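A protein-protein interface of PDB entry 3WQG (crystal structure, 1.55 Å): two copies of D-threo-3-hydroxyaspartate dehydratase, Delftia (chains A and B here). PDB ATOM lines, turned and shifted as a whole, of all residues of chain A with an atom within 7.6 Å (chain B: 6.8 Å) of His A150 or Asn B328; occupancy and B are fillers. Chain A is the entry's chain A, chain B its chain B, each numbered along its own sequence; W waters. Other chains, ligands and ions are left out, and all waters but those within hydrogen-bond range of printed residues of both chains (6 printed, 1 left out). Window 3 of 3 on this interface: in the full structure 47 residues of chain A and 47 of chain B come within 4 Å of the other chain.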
ATOM      1  N   LYS A  53      -1.292 -11.610 -28.033  1.00  0.00           N
ATOM      2  CA  LYS A  53      -2.541 -12.384 -28.164  1.00  0.00           C
ATOM      3  C   LYS A  53      -3.697 -11.687 -27.431  1.00  0.00           C
ATOM      4  O   LYS A  53      -4.853 -12.025 -27.704  1.00  0.00           O
ATOM      5  CB  LYS A  53      -2.337 -13.822 -27.669  1.00  0.00           C
ATOM      6  CG  LYS A  53      -2.286 -13.965 -26.140  1.00  0.00           C
ATOM      7  CD  LYS A  53      -2.168 -15.440 -25.809  1.00  0.00           C
ATOM      8  CE  LYS A  53      -2.203 -15.701 -24.272  1.00  0.00           C
ATOM      9  NZ  LYS A  53      -0.963 -16.197 -23.707  1.00  0.00           N
ATOM     10  N   GLU A 144      10.778 -25.101 -24.337  1.00  0.00           N
ATOM     11  CA  GLU A 144       9.798 -24.630 -23.284  1.00  0.00           C
ATOM     12  C   GLU A 144       9.984 -25.490 -22.017  1.00  0.00           C
ATOM     13  O   GLU A 144      10.007 -26.737 -22.132  1.00  0.00           O
ATOM     14  CB  GLU A 144       8.361 -24.763 -23.806  1.00  0.00           C
ATOM     15  CG  GLU A 144       7.377 -24.157 -22.851  1.00  0.00           C
ATOM     16  CD  GLU A 144       5.941 -24.056 -23.384  1.00  0.00           C
ATOM     17  OE1 GLU A 144       5.184 -23.305 -22.651  1.00  0.00           O
ATOM     18  OE2 GLU A 144       5.566 -24.741 -24.361  1.00  0.00           O
ATOM     19  N   ASP A 146       8.490 -26.439 -18.136  1.00  0.00           N
ATOM     20  CA  ASP A 146       7.287 -26.490 -17.321  1.00  0.00           C
ATOM     21  C   ASP A 146       7.808 -26.171 -15.893  1.00  0.00           C
ATOM     22  O   ASP A 146       8.562 -26.971 -15.314  1.00  0.00           O
ATOM     23  CB  ASP A 146       6.666 -27.858 -17.428  1.00  0.00           C
ATOM     24  CG  ASP A 146       5.585 -28.062 -16.398  1.00  0.00           C
ATOM     25  OD1 ASP A 146       5.260 -27.055 -15.715  1.00  0.00           O
ATOM     26  OD2 ASP A 146       5.081 -29.181 -16.299  1.00  0.00           O
ATOM     27  N   THR A 147       7.544 -24.979 -15.355  1.00  0.00           N
ATOM     28  CA  THR A 147       8.062 -24.627 -14.020  1.00  0.00           C
ATOM     29  C   THR A 147       6.999 -24.702 -12.924  1.00  0.00           C
ATOM     30  O   THR A 147       7.353 -24.535 -11.728  1.00  0.00           O
ATOM     31  CB  THR A 147       8.687 -23.213 -13.943  1.00  0.00           C
ATOM     32  OG1 THR A 147       7.782 -22.244 -14.506  1.00  0.00           O
ATOM     33  CG2 THR A 147      10.085 -23.110 -14.705  1.00  0.00           C
ATOM     34  N   ASP A 148       5.728 -24.923 -13.330  1.00  0.00           N
ATOM     35  CA  ASP A 148       4.639 -24.917 -12.378  1.00  0.00           C
ATOM     36  C   ASP A 148       3.478 -25.935 -12.606  1.00  0.00           C
ATOM     37  O   ASP A 148       2.504 -25.888 -11.860  1.00  0.00           O
ATOM     38  CB  ASP A 148       4.052 -23.501 -12.287  1.00  0.00           C
ATOM     39  CG  ASP A 148       3.279 -23.127 -13.540  1.00  0.00           C
ATOM     40  OD1 ASP A 148       3.336 -23.844 -14.553  1.00  0.00           O
ATOM     41  OD2 ASP A 148       2.551 -22.133 -13.500  1.00  0.00           O
ATOM     42  N   GLY A 149       3.611 -26.859 -13.561  1.00  0.00           N
ATOM     43  CA  GLY A 149       2.595 -27.859 -13.898  1.00  0.00           C
ATOM     44  C   GLY A 149       1.381 -27.323 -14.615  1.00  0.00           C
ATOM     45  O   GLY A 149       0.361 -28.003 -14.699  1.00  0.00           O
ATOM     46  N   HIS A 150       1.489 -26.119 -15.196  1.00  0.00           N
ATOM     47  CA  HIS A 150       0.324 -25.491 -15.786  1.00  0.00           C
ATOM     48  C   HIS A 150      -0.094 -26.065 -17.114  1.00  0.00           C
ATOM     49  O   HIS A 150      -1.267 -26.201 -17.382  1.00  0.00           O
ATOM     50  CB  HIS A 150       0.694 -23.984 -15.956  1.00  0.00           C
ATOM     51  CG  HIS A 150      -0.356 -23.163 -16.598  1.00  0.00           C
ATOM     52  ND1 HIS A 150      -1.593 -22.952 -16.012  1.00  0.00           N
ATOM     53  CD2 HIS A 150      -0.349 -22.478 -17.824  1.00  0.00           C
ATOM     54  CE1 HIS A 150      -2.327 -22.158 -16.874  1.00  0.00           C
ATOM     55  NE2 HIS A 150      -1.552 -21.863 -17.951  1.00  0.00           N
ATOM     56  N   ARG A 151       0.859 -26.367 -17.996  1.00  0.00           N
ATOM     57  CA  ARG A 151       0.515 -26.583 -19.425  1.00  0.00           C
ATOM     58  C   ARG A 151       1.674 -27.377 -20.114  1.00  0.00           C
ATOM     59  O   ARG A 151       2.032 -28.501 -19.649  1.00  0.00           O
ATOM     60  CB  ARG A 151       0.303 -25.199 -20.112  1.00  0.00           C
ATOM     61  CG  ARG A 151      -0.515 -25.291 -21.400  1.00  0.00           C
ATOM     62  CD  ARG A 151      -1.049 -23.914 -21.745  1.00  0.00           C
ATOM     63  NE  ARG A 151       0.046 -23.008 -22.155  1.00  0.00           N
ATOM     64  CZ  ARG A 151      -0.107 -21.677 -22.210  1.00  0.00           C
ATOM     65  NH1 ARG A 151      -1.247 -21.121 -21.680  1.00  0.00           N
ATOM     66  NH2 ARG A 151       0.929 -20.905 -22.696  1.00  0.00           N
ATOM     67  N   SER A 152       2.301 -26.791 -21.148  1.00  0.00           N
ATOM     68  CA  SER A 152       3.357 -27.501 -21.935  1.00  0.00           C
ATOM     69  C   SER A 152       4.713 -27.335 -21.249  1.00  0.00           C
ATOM     70  O   SER A 152       4.879 -26.599 -20.229  1.00  0.00           O
ATOM     71  CB  SER A 152       3.528 -26.933 -23.348  1.00  0.00           C
ATOM     72  OG  SER A 152       2.330 -26.862 -24.026  1.00  0.00           O
ATOM     73  N   HIS A 182       6.271 -20.234 -18.868  1.00  0.00           N
ATOM     74  CA  HIS A 182       5.117 -19.372 -18.569  1.00  0.00           C
ATOM     75  C   HIS A 182       4.462 -19.971 -17.344  1.00  0.00           C
ATOM     76  O   HIS A 182       3.861 -21.069 -17.465  1.00  0.00           O
ATOM     77  CB  HIS A 182       4.176 -19.421 -19.796  1.00  0.00           C
ATOM     78  CG  HIS A 182       2.810 -18.805 -19.576  1.00  0.00           C
ATOM     79  ND1 HIS A 182       2.618 -17.484 -19.300  1.00  0.00           N
ATOM     80  CD2 HIS A 182       1.524 -19.410 -19.641  1.00  0.00           C
ATOM     81  CE1 HIS A 182       1.229 -17.245 -19.209  1.00  0.00           C
ATOM     82  NE2 HIS A 182       0.588 -18.417 -19.458  1.00  0.00           N
ATOM     83  N   ALA A 183       4.488 -19.244 -16.217  1.00  0.00           N
ATOM     84  CA  ALA A 183       3.915 -19.790 -14.976  1.00  0.00           C
ATOM     85  C   ALA A 183       2.411 -19.331 -14.919  1.00  0.00           C
ATOM     86  O   ALA A 183       1.996 -18.483 -14.078  1.00  0.00           O
ATOM     87  CB  ALA A 183       4.675 -19.343 -13.758  1.00  0.00           C
ATOM     88  N   GLY A 184       1.594 -19.843 -15.852  1.00  0.00           N
ATOM     89  CA  GLY A 184       0.203 -19.454 -15.958  1.00  0.00           C
ATOM     90  C   GLY A 184      -0.617 -19.937 -14.776  1.00  0.00           C
ATOM     91  O   GLY A 184      -1.773 -19.488 -14.620  1.00  0.00           O
ATOM     92  N   SER A 185      -0.101 -20.841 -13.921  1.00  0.00           N
ATOM     93  CA  SER A 185      -0.840 -21.171 -12.677  1.00  0.00           C
ATOM     94  C   SER A 185      -1.005 -19.945 -11.750  1.00  0.00           C
ATOM     95  O   SER A 185      -1.796 -19.963 -10.777  1.00  0.00           O
ATOM     96  CB  SER A 185      -0.172 -22.324 -11.922  1.00  0.00           C
ATOM     97  OG  SER A 185       1.033 -21.857 -11.286  1.00  0.00           O
ATOM     98  N   SER A 186      -0.304 -18.839 -12.070  1.00  0.00           N
ATOM     99  CA  SER A 186      -0.432 -17.559 -11.305  1.00  0.00           C
ATOM    100  C   SER A 186      -1.902 -17.083 -11.320  1.00  0.00           C
ATOM    101  O   SER A 186      -2.337 -16.378 -10.365  1.00  0.00           O
ATOM    102  CB  SER A 186       0.504 -16.471 -11.840  1.00  0.00           C
ATOM    103  OG  SER A 186       0.071 -16.108 -13.169  1.00  0.00           O
ATOM    104  N   TYR A 187      -2.658 -17.511 -12.311  1.00  0.00           N
ATOM    105  CA  TYR A 187      -4.065 -17.063 -12.427  1.00  0.00           C
ATOM    106  C   TYR A 187      -4.910 -17.623 -11.320  1.00  0.00           C
ATOM    107  O   TYR A 187      -6.014 -17.085 -11.015  1.00  0.00           O
ATOM    108  CB  TYR A 187      -4.626 -17.459 -13.814  1.00  0.00           C
ATOM    109  CG  TYR A 187      -4.234 -16.465 -14.891  1.00  0.00           C
ATOM    110  CD1 TYR A 187      -2.894 -16.188 -15.175  1.00  0.00           C
ATOM    111  CD2 TYR A 187      -5.264 -15.750 -15.610  1.00  0.00           C
ATOM    112  CE1 TYR A 187      -2.547 -15.276 -16.153  1.00  0.00           C
ATOM    113  CE2 TYR A 187      -4.916 -14.786 -16.579  1.00  0.00           C
ATOM    114  CZ  TYR A 187      -3.537 -14.581 -16.842  1.00  0.00           C
ATOM    115  OH  TYR A 187      -3.129 -13.667 -17.789  1.00  0.00           O
ATOM    116  N   GLU A 188      -4.448 -18.670 -10.667  1.00  0.00           N
ATOM    117  CA  GLU A 188      -5.223 -19.253  -9.513  1.00  0.00           C
ATOM    118  C   GLU A 188      -4.902 -18.596  -8.160  1.00  0.00           C
ATOM    119  O   GLU A 188      -5.466 -18.939  -7.132  1.00  0.00           O
ATOM    120  CB  GLU A 188      -4.808 -20.697  -9.362  1.00  0.00           C
ATOM    121  CG  GLU A 188      -5.177 -21.490 -10.581  1.00  0.00           C
ATOM    122  CD  GLU A 188      -4.326 -22.729 -10.701  1.00  0.00           C
ATOM    123  OE1 GLU A 188      -3.845 -23.258  -9.648  1.00  0.00           O
ATOM    124  OE2 GLU A 188      -4.135 -23.171 -11.857  1.00  0.00           O
ATOM    125  N   ARG A 201       9.876 -19.248  -8.355  1.00  0.00           N
ATOM    126  CA  ARG A 201       9.948 -20.639  -8.816  1.00  0.00           C
ATOM    127  C   ARG A 201      10.040 -20.663 -10.357  1.00  0.00           C
ATOM    128  O   ARG A 201      10.787 -21.506 -10.961  1.00  0.00           O
ATOM    129  CB  ARG A 201       8.698 -21.342  -8.310  1.00  0.00           C
ATOM    130  CG  ARG A 201       8.436 -22.740  -8.776  1.00  0.00           C
ATOM    131  CD  ARG A 201       7.316 -23.316  -7.930  1.00  0.00           C
ATOM    132  NE  ARG A 201       6.543 -24.303  -8.681  1.00  0.00           N
ATOM    133  CZ  ARG A 201       6.821 -25.610  -8.715  1.00  0.00           C
ATOM    134  NH1 ARG A 201       7.871 -26.079  -8.039  1.00  0.00           N
ATOM    135  NH2 ARG A 201       6.061 -26.455  -9.421  1.00  0.00           N
ATOM    136  N   HIS A 361     -12.321 -11.252 -18.684  1.00  0.00           N
ATOM    137  CA  HIS A 361     -11.050 -11.671 -19.276  1.00  0.00           C
ATOM    138  C   HIS A 361     -10.859 -10.806 -20.520  1.00  0.00           C
ATOM    139  O   HIS A 361     -11.623 -10.947 -21.526  1.00  0.00           O
ATOM    140  CB  HIS A 361     -11.188 -13.158 -19.651  1.00  0.00           C
ATOM    141  CG  HIS A 361      -9.925 -13.755 -20.199  1.00  0.00           C
ATOM    142  ND1 HIS A 361      -9.639 -15.046 -20.048  1.00  0.00           N
ATOM    143  CD2 HIS A 361      -8.877 -13.216 -20.874  1.00  0.00           C
ATOM    144  CE1 HIS A 361      -8.428 -15.349 -20.600  1.00  0.00           C
ATOM    145  NE2 HIS A 361      -7.918 -14.247 -21.039  1.00  0.00           N
ATOM    146  N   GLN B 278       1.790 -34.333 -21.688  1.00  0.00           N
ATOM    147  CA  GLN B 278       2.406 -34.465 -20.292  1.00  0.00           C
ATOM    148  C   GLN B 278       2.123 -35.879 -19.912  1.00  0.00           C
ATOM    149  O   GLN B 278       1.095 -36.160 -19.283  1.00  0.00           O
ATOM    150  CB  GLN B 278       1.837 -33.432 -19.262  1.00  0.00           C
ATOM    151  CG  GLN B 278       2.259 -31.952 -19.486  1.00  0.00           C
ATOM    152  CD  GLN B 278       3.779 -31.688 -19.460  1.00  0.00           C
ATOM    153  OE1 GLN B 278       4.564 -32.588 -19.194  1.00  0.00           O
ATOM    154  NE2 GLN B 278       4.191 -30.475 -19.796  1.00  0.00           N
ATOM    155  N   LYS B 281       0.842 -37.226 -16.534  1.00  0.00           N
ATOM    156  CA  LYS B 281      -0.485 -36.802 -16.074  1.00  0.00           C
ATOM    157  C   LYS B 281      -1.557 -37.349 -17.007  1.00  0.00           C
ATOM    158  O   LYS B 281      -2.728 -37.052 -16.822  1.00  0.00           O
ATOM    159  CB  LYS B 281      -0.579 -35.262 -16.018  1.00  0.00           C
ATOM    160  CG  LYS B 281       0.305 -34.661 -14.911  1.00  0.00           C
ATOM    161  CD  LYS B 281       0.006 -33.177 -14.664  1.00  0.00           C
ATOM    162  CE  LYS B 281       0.623 -32.247 -15.726  1.00  0.00           C
ATOM    163  NZ  LYS B 281       0.907 -30.893 -15.145  1.00  0.00           N
ATOM    164  N   TRP B 283      -1.907 -36.408 -20.257  1.00  0.00           N
ATOM    165  CA  TRP B 283      -2.411 -35.254 -21.053  1.00  0.00           C
ATOM    166  C   TRP B 283      -1.912 -35.316 -22.434  1.00  0.00           C
ATOM    167  O   TRP B 283      -0.700 -35.511 -22.600  1.00  0.00           O
ATOM    168  CB  TRP B 283      -1.925 -33.899 -20.556  1.00  0.00           C
ATOM    169  CG  TRP B 283      -2.473 -33.423 -19.243  1.00  0.00           C
ATOM    170  CD1 TRP B 283      -3.404 -34.108 -18.371  1.00  0.00           C
ATOM    171  CD2 TRP B 283      -2.119 -32.187 -18.561  1.00  0.00           C
ATOM    172  NE1 TRP B 283      -3.628 -33.357 -17.247  1.00  0.00           N
ATOM    173  CE2 TRP B 283      -2.895 -32.172 -17.302  1.00  0.00           C
ATOM    174  CE3 TRP B 283      -1.286 -31.110 -18.853  1.00  0.00           C
ATOM    175  CZ2 TRP B 283      -2.812 -31.107 -16.400  1.00  0.00           C
ATOM    176  CZ3 TRP B 283      -1.197 -30.056 -17.941  1.00  0.00           C
ATOM    177  CH2 TRP B 283      -1.957 -30.055 -16.734  1.00  0.00           C
ATOM    178  N   ALA B 288      -6.447 -26.719 -30.303  1.00  0.00           N
ATOM    179  CA  ALA B 288      -7.770 -26.121 -30.096  1.00  0.00           C
ATOM    180  C   ALA B 288      -7.887 -25.752 -28.596  1.00  0.00           C
ATOM    181  O   ALA B 288      -8.187 -26.635 -27.758  1.00  0.00           O
ATOM    182  CB  ALA B 288      -8.868 -27.089 -30.523  1.00  0.00           C
ATOM    183  N   GLY B 289      -7.655 -24.474 -28.241  1.00  0.00           N
ATOM    184  CA  GLY B 289      -7.918 -24.020 -26.873  1.00  0.00           C
ATOM    185  C   GLY B 289      -9.247 -23.280 -26.817  1.00  0.00           C
ATOM    186  O   GLY B 289     -10.108 -23.537 -27.689  1.00  0.00           O
ATOM    187  N   TRP B 290      -9.478 -22.434 -25.793  1.00  0.00           N
ATOM    188  CA  TRP B 290     -10.801 -21.770 -25.738  1.00  0.00           C
ATOM    189  C   TRP B 290     -10.988 -20.738 -26.822  1.00  0.00           C
ATOM    190  O   TRP B 290     -12.119 -20.411 -27.192  1.00  0.00           O
ATOM    191  CB  TRP B 290     -11.086 -21.198 -24.352  1.00  0.00           C
ATOM    192  CG  TRP B 290     -10.131 -20.094 -23.895  1.00  0.00           C
ATOM    193  CD1 TRP B 290      -9.149 -20.155 -22.888  1.00  0.00           C
ATOM    194  CD2 TRP B 290     -10.068 -18.680 -24.398  1.00  0.00           C
ATOM    195  NE1 TRP B 290      -8.530 -18.961 -22.751  1.00  0.00           N
ATOM    196  CE2 TRP B 290      -9.021 -18.038 -23.651  1.00  0.00           C
ATOM    197  CE3 TRP B 290     -10.818 -17.897 -25.349  1.00  0.00           C
ATOM    198  CZ2 TRP B 290      -8.724 -16.665 -23.846  1.00  0.00           C
ATOM    199  CZ3 TRP B 290     -10.440 -16.561 -25.599  1.00  0.00           C
ATOM    200  CH2 TRP B 290      -9.422 -15.967 -24.843  1.00  0.00           C
ATOM    201  N   MET B 291      -9.879 -20.219 -27.427  1.00  0.00           N
ATOM    202  CA  MET B 291     -10.091 -19.389 -28.620  1.00  0.00           C
ATOM    203  C   MET B 291     -10.801 -20.139 -29.740  1.00  0.00           C
ATOM    204  O   MET B 291     -11.591 -19.537 -30.466  1.00  0.00           O
ATOM    205  CB  MET B 291      -8.789 -18.703 -29.074  1.00  0.00           C
ATOM    206  CG  MET B 291      -8.995 -17.585 -30.174  1.00  0.00           C
ATOM    207  SD  MET B 291      -9.977 -16.173 -29.512  1.00  0.00           S
ATOM    208  CE  MET B 291      -8.719 -15.405 -28.460  1.00  0.00           C
ATOM    209  N   ALA B 292     -10.534 -21.457 -29.916  1.00  0.00           N
ATOM    210  CA  ALA B 292     -11.238 -22.237 -30.893  1.00  0.00           C
ATOM    211  C   ALA B 292     -12.593 -22.709 -30.346  1.00  0.00           C
ATOM    212  O   ALA B 292     -13.593 -22.634 -31.090  1.00  0.00           O
ATOM    213  CB  ALA B 292     -10.385 -23.456 -31.267  1.00  0.00           C
ATOM    214  N   ARG B 295     -15.235 -20.094 -24.612  1.00  0.00           N
ATOM    215  CA  ARG B 295     -15.275 -20.382 -23.201  1.00  0.00           C
ATOM    216  C   ARG B 295     -16.596 -21.087 -22.727  1.00  0.00           C
ATOM    217  O   ARG B 295     -16.752 -21.355 -21.506  1.00  0.00           O
ATOM    218  CB  ARG B 295     -15.116 -19.092 -22.369  1.00  0.00           C
ATOM    219  CG  ARG B 295     -13.618 -18.763 -22.279  1.00  0.00           C
ATOM    220  CD  ARG B 295     -12.966 -19.771 -21.336  1.00  0.00           C
ATOM    221  NE  ARG B 295     -11.931 -19.053 -20.646  1.00  0.00           N
ATOM    222  CZ  ARG B 295     -10.888 -19.652 -20.070  1.00  0.00           C
ATOM    223  NH1 ARG B 295     -10.842 -20.985 -20.110  1.00  0.00           N
ATOM    224  NH2 ARG B 295      -9.927 -18.938 -19.431  1.00  0.00           N
ATOM    225  N   TYR B 308     -14.296 -28.913 -22.227  1.00  0.00           N
ATOM    226  CA  TYR B 308     -14.316 -28.042 -23.386  1.00  0.00           C
ATOM    227  C   TYR B 308     -14.585 -28.795 -24.722  1.00  0.00           C
ATOM    228  O   TYR B 308     -14.476 -28.208 -25.796  1.00  0.00           O
ATOM    229  CB  TYR B 308     -13.022 -27.258 -23.530  1.00  0.00           C
ATOM    230  CG  TYR B 308     -12.962 -26.163 -22.490  1.00  0.00           C
ATOM    231  CD1 TYR B 308     -12.345 -26.342 -21.203  1.00  0.00           C
ATOM    232  CD2 TYR B 308     -13.505 -24.884 -22.833  1.00  0.00           C
ATOM    233  CE1 TYR B 308     -12.374 -25.297 -20.259  1.00  0.00           C
ATOM    234  CE2 TYR B 308     -13.483 -23.851 -21.917  1.00  0.00           C
ATOM    235  CZ  TYR B 308     -12.953 -24.057 -20.654  1.00  0.00           C
ATOM    236  OH  TYR B 308     -12.940 -22.975 -19.795  1.00  0.00           O
ATOM    237  N   GLY B 326      -9.300 -29.183 -20.040  1.00  0.00           N
ATOM    238  CA  GLY B 326      -8.890 -27.817 -19.678  1.00  0.00           C
ATOM    239  C   GLY B 326      -8.597 -27.126 -20.996  1.00  0.00           C
ATOM    240  O   GLY B 326      -8.526 -27.797 -22.062  1.00  0.00           O
ATOM    241  N   ALA B 327      -8.595 -25.802 -20.923  1.00  0.00           N
ATOM    242  CA  ALA B 327      -8.261 -25.032 -22.087  1.00  0.00           C
ATOM    243  C   ALA B 327      -7.624 -23.730 -21.755  1.00  0.00           C
ATOM    244  O   ALA B 327      -8.144 -22.960 -20.887  1.00  0.00           O
ATOM    245  CB  ALA B 327      -9.483 -24.796 -22.993  1.00  0.00           C
ATOM    246  N   ASN B 328      -6.526 -23.438 -22.463  1.00  0.00           N
ATOM    247  CA  ASN B 328      -6.055 -22.066 -22.426  1.00  0.00           C
ATOM    248  C   ASN B 328      -6.302 -21.431 -23.775  1.00  0.00           C
ATOM    249  O   ASN B 328      -6.998 -22.028 -24.572  1.00  0.00           O
ATOM    250  CB  ASN B 328      -4.604 -21.993 -21.977  1.00  0.00           C
ATOM    251  CG  ASN B 328      -4.444 -22.234 -20.428  1.00  0.00           C
ATOM    252  OD1 ASN B 328      -3.390 -22.400 -19.982  1.00  0.00           O
ATOM    253  ND2 ASN B 328      -5.539 -22.211 -19.647  1.00  0.00           N
ATOM    254  N   GLN B 329      -5.721 -20.273 -24.048  1.00  0.00           N
ATOM    255  CA  GLN B 329      -6.180 -19.542 -25.219  1.00  0.00           C
ATOM    256  C   GLN B 329      -6.017 -20.373 -26.519  1.00  0.00           C
ATOM    257  O   GLN B 329      -6.952 -20.545 -27.335  1.00  0.00           O
ATOM    258  CB  GLN B 329      -5.498 -18.186 -25.290  1.00  0.00           C
ATOM    259  CG  GLN B 329      -6.124 -17.274 -26.326  1.00  0.00           C
ATOM    260  CD  GLN B 329      -5.729 -15.811 -26.101  1.00  0.00           C
ATOM    261  OE1 GLN B 329      -5.573 -15.339 -24.957  1.00  0.00           O
ATOM    262  NE2 GLN B 329      -5.613 -15.081 -27.231  1.00  0.00           N
ATOM    263  N   GLU B 330      -4.784 -20.843 -26.743  1.00  0.00           N
ATOM    264  CA  GLU B 330      -4.466 -21.572 -27.963  1.00  0.00           C
ATOM    265  C   GLU B 330      -4.010 -23.044 -27.722  1.00  0.00           C
ATOM    266  O   GLU B 330      -3.522 -23.697 -28.637  1.00  0.00           O
ATOM    267  CB  GLU B 330      -3.429 -20.836 -28.817  1.00  0.00           C
ATOM    268  CG  GLU B 330      -3.975 -19.549 -29.436  1.00  0.00           C
ATOM    269  CD  GLU B 330      -5.051 -19.747 -30.497  1.00  0.00           C
ATOM    270  OE1 GLU B 330      -5.251 -20.858 -31.073  1.00  0.00           O
ATOM    271  OE2 GLU B 330      -5.825 -18.758 -30.697  1.00  0.00           O
ATOM    272  N   HIS B 331      -4.221 -23.527 -26.494  1.00  0.00           N
ATOM    273  CA  HIS B 331      -3.892 -24.905 -26.127  1.00  0.00           C
ATOM    274  C   HIS B 331      -5.090 -25.517 -25.485  1.00  0.00           C
ATOM    275  O   HIS B 331      -5.612 -24.954 -24.492  1.00  0.00           O
ATOM    276  CB  HIS B 331      -2.865 -24.947 -24.953  1.00  0.00           C
ATOM    277  CG  HIS B 331      -1.552 -24.277 -25.208  1.00  0.00           C
ATOM    278  ND1 HIS B 331      -1.382 -22.898 -25.263  1.00  0.00           N
ATOM    279  CD2 HIS B 331      -0.305 -24.829 -25.389  1.00  0.00           C
ATOM    280  CE1 HIS B 331      -0.068 -22.610 -25.454  1.00  0.00           C
ATOM    281  NE2 HIS B 331       0.605 -23.791 -25.520  1.00  0.00           N
ATOM    282  N   GLY B 332      -5.456 -26.718 -25.880  1.00  0.00           N
ATOM    283  CA  GLY B 332      -6.467 -27.507 -25.167  1.00  0.00           C
ATOM    284  C   GLY B 332      -5.776 -28.687 -24.503  1.00  0.00           C
ATOM    285  O   GLY B 332      -4.820 -29.263 -25.057  1.00  0.00           O
ATOM    286  N   ILE B 333      -6.274 -29.093 -23.334  1.00  0.00           N
ATOM    287  CA  ILE B 333      -5.690 -30.225 -22.595  1.00  0.00           C
ATOM    288  C   ILE B 333      -6.669 -31.380 -22.763  1.00  0.00           C
ATOM    289  O   ILE B 333      -7.830 -31.296 -22.292  1.00  0.00           O
ATOM    290  CB  ILE B 333      -5.539 -29.905 -21.072  1.00  0.00           C
ATOM    291  CG1 ILE B 333      -4.779 -28.579 -20.719  1.00  0.00           C
ATOM    292  CG2 ILE B 333      -5.062 -31.191 -20.330  1.00  0.00           C
ATOM    293  CD1 ILE B 333      -3.482 -28.503 -21.370  1.00  0.00           C
HETATM  294  O   HOH W   1       3.142 -21.967 -24.403  1.00  0.00           O
HETATM  295  O   HOH W   2       3.229 -24.674 -25.801  1.00  0.00           O
HETATM  296  O   HOH W   3      -5.392 -15.886 -22.334  1.00  0.00           O
HETATM  297  O   HOH W   4       6.300 -31.338 -17.078  1.00  0.00           O
HETATM  298  O   HOH W   5      -3.456 -25.041 -18.941  1.00  0.00           O
HETATM  299  O   HOH W   6      -1.227 -30.313 -13.257  1.00  0.00           O
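The backbone carbonyl oxygen of Asn B328 sits at hydrogen-bond distance from the backbone NH of Trp B290, 2.8 Å away.
The backbone NH (N) of Gly A149 sits at hydrogen-bond distance from the side-chain carboxylate (OD1) of Asp A146 (2.7 Å).
OD1 of Asp A146 lies within hydrogen-bond range of N of Asp A148 (3.2 Å).
O of Ala B327 is in hydrogen-bond range of NH1 of Arg B295.
The backbone NH of Gln B278 lies within hydrogen-bond range of the backbone carbonyl oxygen of Trp B283 (2.9 Å).
The side-chain hydroxyl of Tyr B308 sits at hydrogen-bond distance from the guanidinium group of Arg B295.
Water W4 lies within hydrogen-bond range of OD2 of Asp A146 (2.6 Å) and OE1 of Gln B278 (3.0 Å).
Water W3 lies within hydrogen-bond range of the side-chain amide oxygen (OE1) of Gln B329 and a ring nitrogen (NE2) of His A361.
Water W2 lies within hydrogen-bond range of the side-chain carboxylate (OE2) of Glu A144 (2.7 Å), a ring nitrogen (NE2) of His B331 (2.8 Å) and the side-chain hydroxyl (OG) of Ser A152 (3.0 Å).
Water W5 bridges the side-chain amide oxygen (OD1) of Asn B328 (2.8 Å) and the backbone carbonyl oxygen (O) of His A150 (2.9 Å).
Water W6 lies within hydrogen-bond range of the side-chain amino group (NZ) of Lys B281 (2.9 Å) and the backbone carbonyl oxygen (O) of Gly A149 (3.2 Å).
Water W1 lies within hydrogen-bond range of NH2 of Arg A151 (3.0 Å), OE1 of Glu A144 (3.0 Å) and NE2 of His B331 (3.3 Å).
Printed residues of chain A that touch a printed residue of chain B: Lys A53, Asp A146, Gly A149, His A150, Arg A151, Ser A152 and His A361.
Among the printed residues, 14 pairs touch across the chains.
Among the printed residues, no Asp or Glu carboxylate lies within 4 Å of a Lys or Arg side-chain nitrogen of the other chain.
No position is printed for both chains.
Among the printed residues, pairs that only touch across the chains: Asp A146 with Gln B278 (3.8 Å), Gly A149 with Trp B283 (3.7 Å), His A150 with Trp B283 (3.9 Å), Arg A151 with Trp B283 (3.97 Å), Ser A152 with Gln B278 (3.5 Å), Ser A152 with His B331 (3.6 Å), His A361 with Trp B290 (3.5 Å) and His A361 with Arg B295 (3.95 Å).
The side-chain amino group (NZ) of Lys B281 sits at hydrogen-bond distance from the backbone carbonyl oxygen (O) of Gly A149 (3.0 Å).
The side-chain amide oxygen of Asn B328 lies within hydrogen-bond range of the guanidinium group of Arg A151.
O of Arg A151 sits at hydrogen-bond distance from NE2 of Gln B278 (2.9 Å).
The side-chain amide oxygen (OD1) of Asn B328 is in hydrogen-bond range of a ring nitrogen (NE2) of His A150, 2.8 Å away.
The guanidinium group (NE) of Arg A151 sits close to a ring nitrogen (ND1) of His B331.
O of Lys A53 lies within hydrogen-bond range of NE2 of Gln B329, at 3.2 Å.
Printed residues of chain B within 4 Å of Lys A53: Gln B329 (3.2 Å).
Glu A144 touches none of the printed residues of chain B.
Of the printed residues of chain B, Asp A146 touches Gln B278 (3.8 Å).
Of chain B, only Trp B283 (3.9 Å) and Asn B328 (2.8 Å) come within 4 Å of His A150.
No residue of chain A comes within 4 Å of Ala B327.
Asn B328 touches just these residues of chain A: His A150 and Arg A151.
Of the printed residues of chain A, Gln B329 touches Lys A53 (3.2 Å).
Of the printed residues of chain A, His B331 touches Arg A151 (3.3 Å) and Ser A152 (3.6 Å).
The nearest residue of chain B that does not touch His A150 is Lys B281 (4.8 Å).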
